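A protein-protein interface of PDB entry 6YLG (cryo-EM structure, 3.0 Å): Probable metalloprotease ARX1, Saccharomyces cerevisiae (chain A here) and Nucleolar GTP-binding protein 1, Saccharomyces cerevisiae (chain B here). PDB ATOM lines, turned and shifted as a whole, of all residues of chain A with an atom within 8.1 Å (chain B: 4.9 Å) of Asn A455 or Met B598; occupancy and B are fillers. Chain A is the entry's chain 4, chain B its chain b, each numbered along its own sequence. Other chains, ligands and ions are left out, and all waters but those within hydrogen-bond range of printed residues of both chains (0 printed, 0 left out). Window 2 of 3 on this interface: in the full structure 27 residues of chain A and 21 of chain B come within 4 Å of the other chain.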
ATOM      1  N   THR A 452      -4.484 -22.001  -0.207  1.00  0.00           N
ATOM      2  CA  THR A 452      -5.397 -21.018  -0.784  1.00  0.00           C
ATOM      3  C   THR A 452      -4.561 -19.988  -1.533  1.00  0.00           C
ATOM      4  O   THR A 452      -3.779 -19.254  -0.920  1.00  0.00           O
ATOM      5  CB  THR A 452      -6.260 -20.353   0.290  1.00  0.00           C
ATOM      6  OG1 THR A 452      -6.910 -19.198  -0.258  1.00  0.00           O
ATOM      7  CG2 THR A 452      -5.428 -19.950   1.501  1.00  0.00           C
ATOM      8  N   ASN A 453      -4.730 -19.937  -2.852  1.00  0.00           N
ATOM      9  CA  ASN A 453      -4.030 -18.997  -3.723  1.00  0.00           C
ATOM     10  C   ASN A 453      -5.043 -18.102  -4.435  1.00  0.00           C
ATOM     11  O   ASN A 453      -5.515 -18.449  -5.521  1.00  0.00           O
ATOM     12  CB  ASN A 453      -3.175 -19.733  -4.756  1.00  0.00           C
ATOM     13  CG  ASN A 453      -3.856 -20.960  -5.324  1.00  0.00           C
ATOM     14  OD1 ASN A 453      -4.545 -21.689  -4.610  1.00  0.00           O
ATOM     15  ND2 ASN A 453      -3.657 -21.203  -6.612  1.00  0.00           N
ATOM     16  N   PRO A 454      -5.414 -16.947  -3.873  1.00  0.00           N
ATOM     17  CA  PRO A 454      -6.515 -16.154  -4.438  1.00  0.00           C
ATOM     18  C   PRO A 454      -6.314 -15.665  -5.864  1.00  0.00           C
ATOM     19  O   PRO A 454      -7.271 -15.158  -6.455  1.00  0.00           O
ATOM     20  CB  PRO A 454      -6.603 -14.962  -3.473  1.00  0.00           C
ATOM     21  CG  PRO A 454      -6.076 -15.467  -2.207  1.00  0.00           C
ATOM     22  CD  PRO A 454      -4.970 -16.392  -2.580  1.00  0.00           C
ATOM     23  N   ASN A 455      -5.120 -15.789  -6.441  1.00  0.00           N
ATOM     24  CA  ASN A 455      -4.925 -15.488  -7.856  1.00  0.00           C
ATOM     25  C   ASN A 455      -3.825 -16.400  -8.376  1.00  0.00           C
ATOM     26  O   ASN A 455      -2.678 -16.307  -7.926  1.00  0.00           O
ATOM     27  CB  ASN A 455      -4.570 -14.016  -8.073  1.00  0.00           C
ATOM     28  CG  ASN A 455      -5.764 -13.167  -8.514  1.00  0.00           C
ATOM     29  OD1 ASN A 455      -6.887 -13.652  -8.657  1.00  0.00           O
ATOM     30  ND2 ASN A 455      -5.510 -11.887  -8.741  1.00  0.00           N
ATOM     31  N   GLY A 456      -4.180 -17.270  -9.314  1.00  0.00           N
ATOM     32  CA  GLY A 456      -3.263 -18.244  -9.884  1.00  0.00           C
ATOM     33  C   GLY A 456      -2.930 -17.875 -11.317  1.00  0.00           C
ATOM     34  O   GLY A 456      -3.778 -17.347 -12.041  1.00  0.00           O
ATOM     35  N   ASN A 457      -1.675 -18.128 -11.700  1.00  0.00           N
ATOM     36  CA  ASN A 457      -1.120 -17.810 -13.014  1.00  0.00           C
ATOM     37  C   ASN A 457      -0.858 -16.317 -13.201  1.00  0.00           C
ATOM     38  O   ASN A 457      -0.326 -15.914 -14.240  1.00  0.00           O
ATOM     39  CB  ASN A 457      -2.027 -18.311 -14.145  1.00  0.00           C
ATOM     40  CG  ASN A 457      -2.502 -19.731 -13.931  1.00  0.00           C
ATOM     41  OD1 ASN A 457      -2.028 -20.428 -13.037  1.00  0.00           O
ATOM     42  ND2 ASN A 457      -3.447 -20.166 -14.753  1.00  0.00           N
ATOM     43  N   LEU A 458      -1.214 -15.491 -12.212  1.00  0.00           N
ATOM     44  CA  LEU A 458      -1.058 -14.046 -12.281  1.00  0.00           C
ATOM     45  C   LEU A 458      -0.127 -13.503 -11.208  1.00  0.00           C
ATOM     46  O   LEU A 458       0.212 -12.315 -11.246  1.00  0.00           O
ATOM     47  CB  LEU A 458      -2.426 -13.367 -12.161  1.00  0.00           C
ATOM     48  CG  LEU A 458      -3.492 -13.811 -13.165  1.00  0.00           C
ATOM     49  CD1 LEU A 458      -4.844 -13.258 -12.769  1.00  0.00           C
ATOM     50  CD2 LEU A 458      -3.128 -13.384 -14.582  1.00  0.00           C
ATOM     51  N   SER A 459       0.290 -14.328 -10.252  1.00  0.00           N
ATOM     52  CA  SER A 459       1.186 -13.882  -9.198  1.00  0.00           C
ATOM     53  C   SER A 459       2.616 -13.840  -9.721  1.00  0.00           C
ATOM     54  O   SER A 459       3.232 -14.887  -9.944  1.00  0.00           O
ATOM     55  CB  SER A 459       1.089 -14.808  -7.989  1.00  0.00           C
ATOM     56  OG  SER A 459      -0.248 -14.928  -7.542  1.00  0.00           O
ATOM     57  N   TYR A 460       3.140 -12.633  -9.919  1.00  0.00           N
ATOM     58  CA  TYR A 460       4.571 -12.454 -10.096  1.00  0.00           C
ATOM     59  C   TYR A 460       5.248 -12.512  -8.730  1.00  0.00           C
ATOM     60  O   TYR A 460       4.637 -12.875  -7.720  1.00  0.00           O
ATOM     61  CB  TYR A 460       4.881 -11.126 -10.789  1.00  0.00           C
ATOM     62  CG  TYR A 460       4.150 -10.857 -12.084  1.00  0.00           C
ATOM     63  CD1 TYR A 460       3.748 -11.891 -12.918  1.00  0.00           C
ATOM     64  CD2 TYR A 460       3.893  -9.554 -12.487  1.00  0.00           C
ATOM     65  CE1 TYR A 460       3.091 -11.635 -14.107  1.00  0.00           C
ATOM     66  CE2 TYR A 460       3.241  -9.286 -13.671  1.00  0.00           C
ATOM     67  CZ  TYR A 460       2.842 -10.329 -14.480  1.00  0.00           C
ATOM     68  OH  TYR A 460       2.191 -10.063 -15.664  1.00  0.00           O
ATOM     69  N   ALA A 462       7.813  -9.664  -8.237  1.00  0.00           N
ATOM     70  CA  ALA A 462       7.683  -8.208  -8.166  1.00  0.00           C
ATOM     71  C   ALA A 462       8.529  -7.606  -7.047  1.00  0.00           C
ATOM     72  O   ALA A 462       8.012  -7.357  -5.952  1.00  0.00           O
ATOM     73  CB  ALA A 462       6.211  -7.795  -8.041  1.00  0.00           C
ATOM     74  N   LEU A 478      -2.859 -26.662 -10.864  1.00  0.00           N
ATOM     75  CA  LEU A 478      -3.043 -26.124  -9.514  1.00  0.00           C
ATOM     76  C   LEU A 478      -2.762 -24.626  -9.427  1.00  0.00           C
ATOM     77  O   LEU A 478      -3.015 -24.014  -8.384  1.00  0.00           O
ATOM     78  CB  LEU A 478      -2.167 -26.847  -8.485  1.00  0.00           C
ATOM     79  CG  LEU A 478      -2.048 -28.367  -8.543  1.00  0.00           C
ATOM     80  CD1 LEU A 478      -1.398 -28.846  -7.263  1.00  0.00           C
ATOM     81  CD2 LEU A 478      -3.403 -29.024  -8.754  1.00  0.00           C
ATOM     82  N   GLY A 479      -2.262 -24.021 -10.501  1.00  0.00           N
ATOM     83  CA  GLY A 479      -2.187 -22.575 -10.609  1.00  0.00           C
ATOM     84  C   GLY A 479      -1.403 -21.847  -9.536  1.00  0.00           C
ATOM     85  O   GLY A 479      -1.709 -20.685  -9.245  1.00  0.00           O
ATOM     86  N   VAL A 480      -0.402 -22.496  -8.938  1.00  0.00           N
ATOM     87  CA  VAL A 480       0.475 -21.980  -7.892  1.00  0.00           C
ATOM     88  C   VAL A 480       1.776 -21.512  -8.528  1.00  0.00           C
ATOM     89  O   VAL A 480       2.249 -22.093  -9.513  1.00  0.00           O
ATOM     90  CB  VAL A 480       0.722 -23.042  -6.800  1.00  0.00           C
ATOM     91  CG1 VAL A 480      -0.577 -23.744  -6.438  1.00  0.00           C
ATOM     92  CG2 VAL A 480       1.768 -24.059  -7.222  1.00  0.00           C
ATOM     93  N   SER A 481       2.352 -20.408  -8.064  1.00  0.00           N
ATOM     94  CA  SER A 481       3.630 -19.946  -8.583  1.00  0.00           C
ATOM     95  C   SER A 481       4.727 -20.104  -7.539  1.00  0.00           C
ATOM     96  O   SER A 481       4.491 -20.549  -6.412  1.00  0.00           O
ATOM     97  CB  SER A 481       3.541 -18.483  -9.016  1.00  0.00           C
ATOM     98  OG  SER A 481       4.732 -18.083  -9.667  1.00  0.00           O
ATOM     99  N   ILE A 483       6.259 -17.865  -5.836  1.00  0.00           N
ATOM    100  CA  ILE A 483       6.077 -17.028  -4.647  1.00  0.00           C
ATOM    101  C   ILE A 483       5.198 -17.738  -3.617  1.00  0.00           C
ATOM    102  O   ILE A 483       5.565 -17.864  -2.440  1.00  0.00           O
ATOM    103  CB  ILE A 483       5.522 -15.638  -5.034  1.00  0.00           C
ATOM    104  CG1 ILE A 483       5.093 -14.857  -3.790  1.00  0.00           C
ATOM    105  CG2 ILE A 483       4.358 -15.700  -6.050  1.00  0.00           C
ATOM    106  CD1 ILE A 483       5.052 -13.362  -4.012  1.00  0.00           C
ATOM    107  N   LYS A 484       4.037 -18.236  -4.044  1.00  0.00           N
ATOM    108  CA  LYS A 484       3.157 -18.926  -3.108  1.00  0.00           C
ATOM    109  C   LYS A 484       3.755 -20.260  -2.685  1.00  0.00           C
ATOM    110  O   LYS A 484       3.508 -20.734  -1.571  1.00  0.00           O
ATOM    111  CB  LYS A 484       1.773 -19.117  -3.731  1.00  0.00           C
ATOM    112  CG  LYS A 484       0.775 -19.949  -2.909  1.00  0.00           C
ATOM    113  CD  LYS A 484       0.549 -19.406  -1.495  1.00  0.00           C
ATOM    114  CE  LYS A 484      -0.314 -20.343  -0.669  1.00  0.00           C
ATOM    115  NZ  LYS A 484      -1.592 -19.719  -0.252  1.00  0.00           N
ATOM    116  N   VAL B 593       3.487  -4.189  -0.796  1.00  0.00           N
ATOM    117  CA  VAL B 593       2.863  -5.108  -1.741  1.00  0.00           C
ATOM    118  C   VAL B 593       3.957  -5.873  -2.470  1.00  0.00           C
ATOM    119  O   VAL B 593       4.790  -5.281  -3.166  1.00  0.00           O
ATOM    120  CB  VAL B 593       1.960  -4.351  -2.725  1.00  0.00           C
ATOM    121  CG1 VAL B 593       1.213  -5.330  -3.629  1.00  0.00           C
ATOM    122  CG2 VAL B 593       0.989  -3.467  -1.970  1.00  0.00           C
ATOM    123  N   ASP B 595       3.414  -8.844  -4.615  1.00  0.00           N
ATOM    124  CA  ASP B 595       3.072  -9.524  -5.857  1.00  0.00           C
ATOM    125  C   ASP B 595       2.370  -8.598  -6.843  1.00  0.00           C
ATOM    126  O   ASP B 595       1.626  -7.685  -6.458  1.00  0.00           O
ATOM    127  CB  ASP B 595       2.202 -10.751  -5.569  1.00  0.00           C
ATOM    128  CG  ASP B 595       0.775 -10.391  -5.276  1.00  0.00           C
ATOM    129  OD1 ASP B 595       0.545  -9.619  -4.323  1.00  0.00           O
ATOM    130  OD2 ASP B 595      -0.116 -10.889  -5.992  1.00  0.00           O
ATOM    131  N   GLY B 596       2.592  -8.879  -8.130  1.00  0.00           N
ATOM    132  CA  GLY B 596       2.163  -7.971  -9.179  1.00  0.00           C
ATOM    133  C   GLY B 596       0.667  -7.977  -9.417  1.00  0.00           C
ATOM    134  O   GLY B 596       0.106  -6.975  -9.863  1.00  0.00           O
ATOM    135  N   SER B 597       0.000  -9.097  -9.135  1.00  0.00           N
ATOM    136  CA  SER B 597      -1.449  -9.137  -9.302  1.00  0.00           C
ATOM    137  C   SER B 597      -2.133  -8.142  -8.370  1.00  0.00           C
ATOM    138  O   SER B 597      -2.942  -7.314  -8.808  1.00  0.00           O
ATOM    139  CB  SER B 597      -1.962 -10.552  -9.054  1.00  0.00           C
ATOM    140  OG  SER B 597      -1.207 -11.195  -8.047  1.00  0.00           O
ATOM    141  N   MET B 598      -1.801  -8.174  -7.080  1.00  0.00           N
ATOM    142  CA  MET B 598      -2.356  -7.194  -6.157  1.00  0.00           C
ATOM    143  C   MET B 598      -1.781  -5.803  -6.390  1.00  0.00           C
ATOM    144  O   MET B 598      -2.451  -4.809  -6.083  1.00  0.00           O
ATOM    145  CB  MET B 598      -2.111  -7.639  -4.714  1.00  0.00           C
ATOM    146  CG  MET B 598      -2.555  -9.067  -4.406  1.00  0.00           C
ATOM    147  SD  MET B 598      -4.131  -9.576  -5.124  1.00  0.00           S
ATOM    148  CE  MET B 598      -3.760 -11.270  -5.579  1.00  0.00           C
ATOM    149  N   ARG B 599      -0.575  -5.705  -6.948  1.00  0.00           N
ATOM    150  CA  ARG B 599      -0.067  -4.395  -7.348  1.00  0.00           C
ATOM    151  C   ARG B 599      -0.972  -3.762  -8.404  1.00  0.00           C
ATOM    152  O   ARG B 599      -1.354  -2.589  -8.297  1.00  0.00           O
ATOM    153  CB  ARG B 599       1.362  -4.540  -7.870  1.00  0.00           C
ATOM    154  CG  ARG B 599       2.318  -3.490  -7.380  1.00  0.00           C
ATOM    155  CD  ARG B 599       3.751  -3.871  -7.705  1.00  0.00           C
ATOM    156  NE  ARG B 599       4.494  -4.216  -6.498  1.00  0.00           N
ATOM    157  CZ  ARG B 599       5.820  -4.206  -6.382  1.00  0.00           C
ATOM    158  NH1 ARG B 599       6.601  -3.870  -7.402  1.00  0.00           N
ATOM    159  NH2 ARG B 599       6.372  -4.533  -5.224  1.00  0.00           N
ATOM    160  N   SER B 600      -1.343  -4.541  -9.419  1.00  0.00           N
ATOM    161  CA  SER B 600      -2.283  -4.086 -10.438  1.00  0.00           C
ATOM    162  C   SER B 600      -3.664  -3.822  -9.859  1.00  0.00           C
ATOM    163  O   SER B 600      -4.338  -2.885 -10.297  1.00  0.00           O
ATOM    164  CB  SER B 600      -2.391  -5.121 -11.554  1.00  0.00           C
ATOM    165  OG  SER B 600      -1.454  -4.869 -12.584  1.00  0.00           O
ATOM    166  N   LYS B 601      -4.095  -4.642  -8.901  1.00  0.00           N
ATOM    167  CA  LYS B 601      -5.345  -4.396  -8.189  1.00  0.00           C
ATOM    168  C   LYS B 601      -5.356  -2.998  -7.573  1.00  0.00           C
ATOM    169  O   LYS B 601      -6.285  -2.209  -7.795  1.00  0.00           O
ATOM    170  CB  LYS B 601      -5.517  -5.477  -7.117  1.00  0.00           C
ATOM    171  CG  LYS B 601      -6.803  -5.467  -6.325  1.00  0.00           C
ATOM    172  CD  LYS B 601      -7.990  -5.903  -7.145  1.00  0.00           C
ATOM    173  CE  LYS B 601      -9.236  -5.957  -6.280  1.00  0.00           C
ATOM    174  NZ  LYS B 601      -9.356  -7.270  -5.593  1.00  0.00           N
ATOM    175  N   ALA B 602      -4.318  -2.677  -6.800  1.00  0.00           N
ATOM    176  CA  ALA B 602      -4.217  -1.361  -6.176  1.00  0.00           C
ATOM    177  C   ALA B 602      -4.158  -0.237  -7.203  1.00  0.00           C
ATOM    178  O   ALA B 602      -4.800   0.807  -7.016  1.00  0.00           O
ATOM    179  CB  ALA B 602      -2.990  -1.308  -5.276  1.00  0.00           C
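The backbone carbonyl oxygen (O) of Ala A462 sits at hydrogen-bond distance from the guanidinium group (NH2) of Arg B599 (3.3 Å).
OG of Ser A459 lies within hydrogen-bond range of O of Asn A455 (2.8 Å).
O of Val B593 lies within hydrogen-bond range of NH2 of Arg B599 (2.7 Å).
N of Met B598 is in hydrogen-bond range of OD2 of Asp B595.
Among the printed residues, merely in contact across the chains: Leu A458 with Ser B597 (3.6 Å), Asn A455 with Met B598 (3.7 Å), Ser A459 with Ser B597 (3.8 Å), Ala A462 with Gly B596 (3.8 Å), Asn A455 with Ser B597 (3.8 Å) and Tyr A460 with Asp B595 (3.9 Å).
Of chain B, only Ser B597 (3.8 Å) and Met B598 (3.7 Å) come within 4 Å of Asn A455.
Of the printed residues of chain B, Ser A459 touches Ser B597 (3.8 Å).
Of the printed residues of chain B, Tyr A460 touches Asp B595 (3.9 Å).
Of the printed residues of chain B, Ala A462 touches Gly B596 (3.8 Å) and Arg B599 (3.3 Å).
Ser B597 touches three residues of chain A.
Of chain A, only Asn A455 comes within 4 Å of Met B598.
Of the printed residues of chain A, Arg B599 touches Ala A462.
The nearest printed residue of chain B that does not touch Asn A455 is Asp B595 (5.8 Å).
The nearest residue of chain A that does not touch Met B598 is Pro A454 (5.1 Å).
Of the 9 printed residues of chain B, 5 touch a printed residue of chain A.
Of the 16 printed residues of chain A, 5 touch a printed residue of chain B.
Printed residues of chain A that touch a printed residue of chain B: Asn A455, Leu A458, Ser A459, Tyr A460 and Ala A462.
Along chain A the printed residues that touch a printed residue of chain B span positions 455 to 462.
Among the printed residues, no Asp or Glu carboxylate lies within 4 Å of a Lys or Arg side-chain nitrogen of the other chain.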
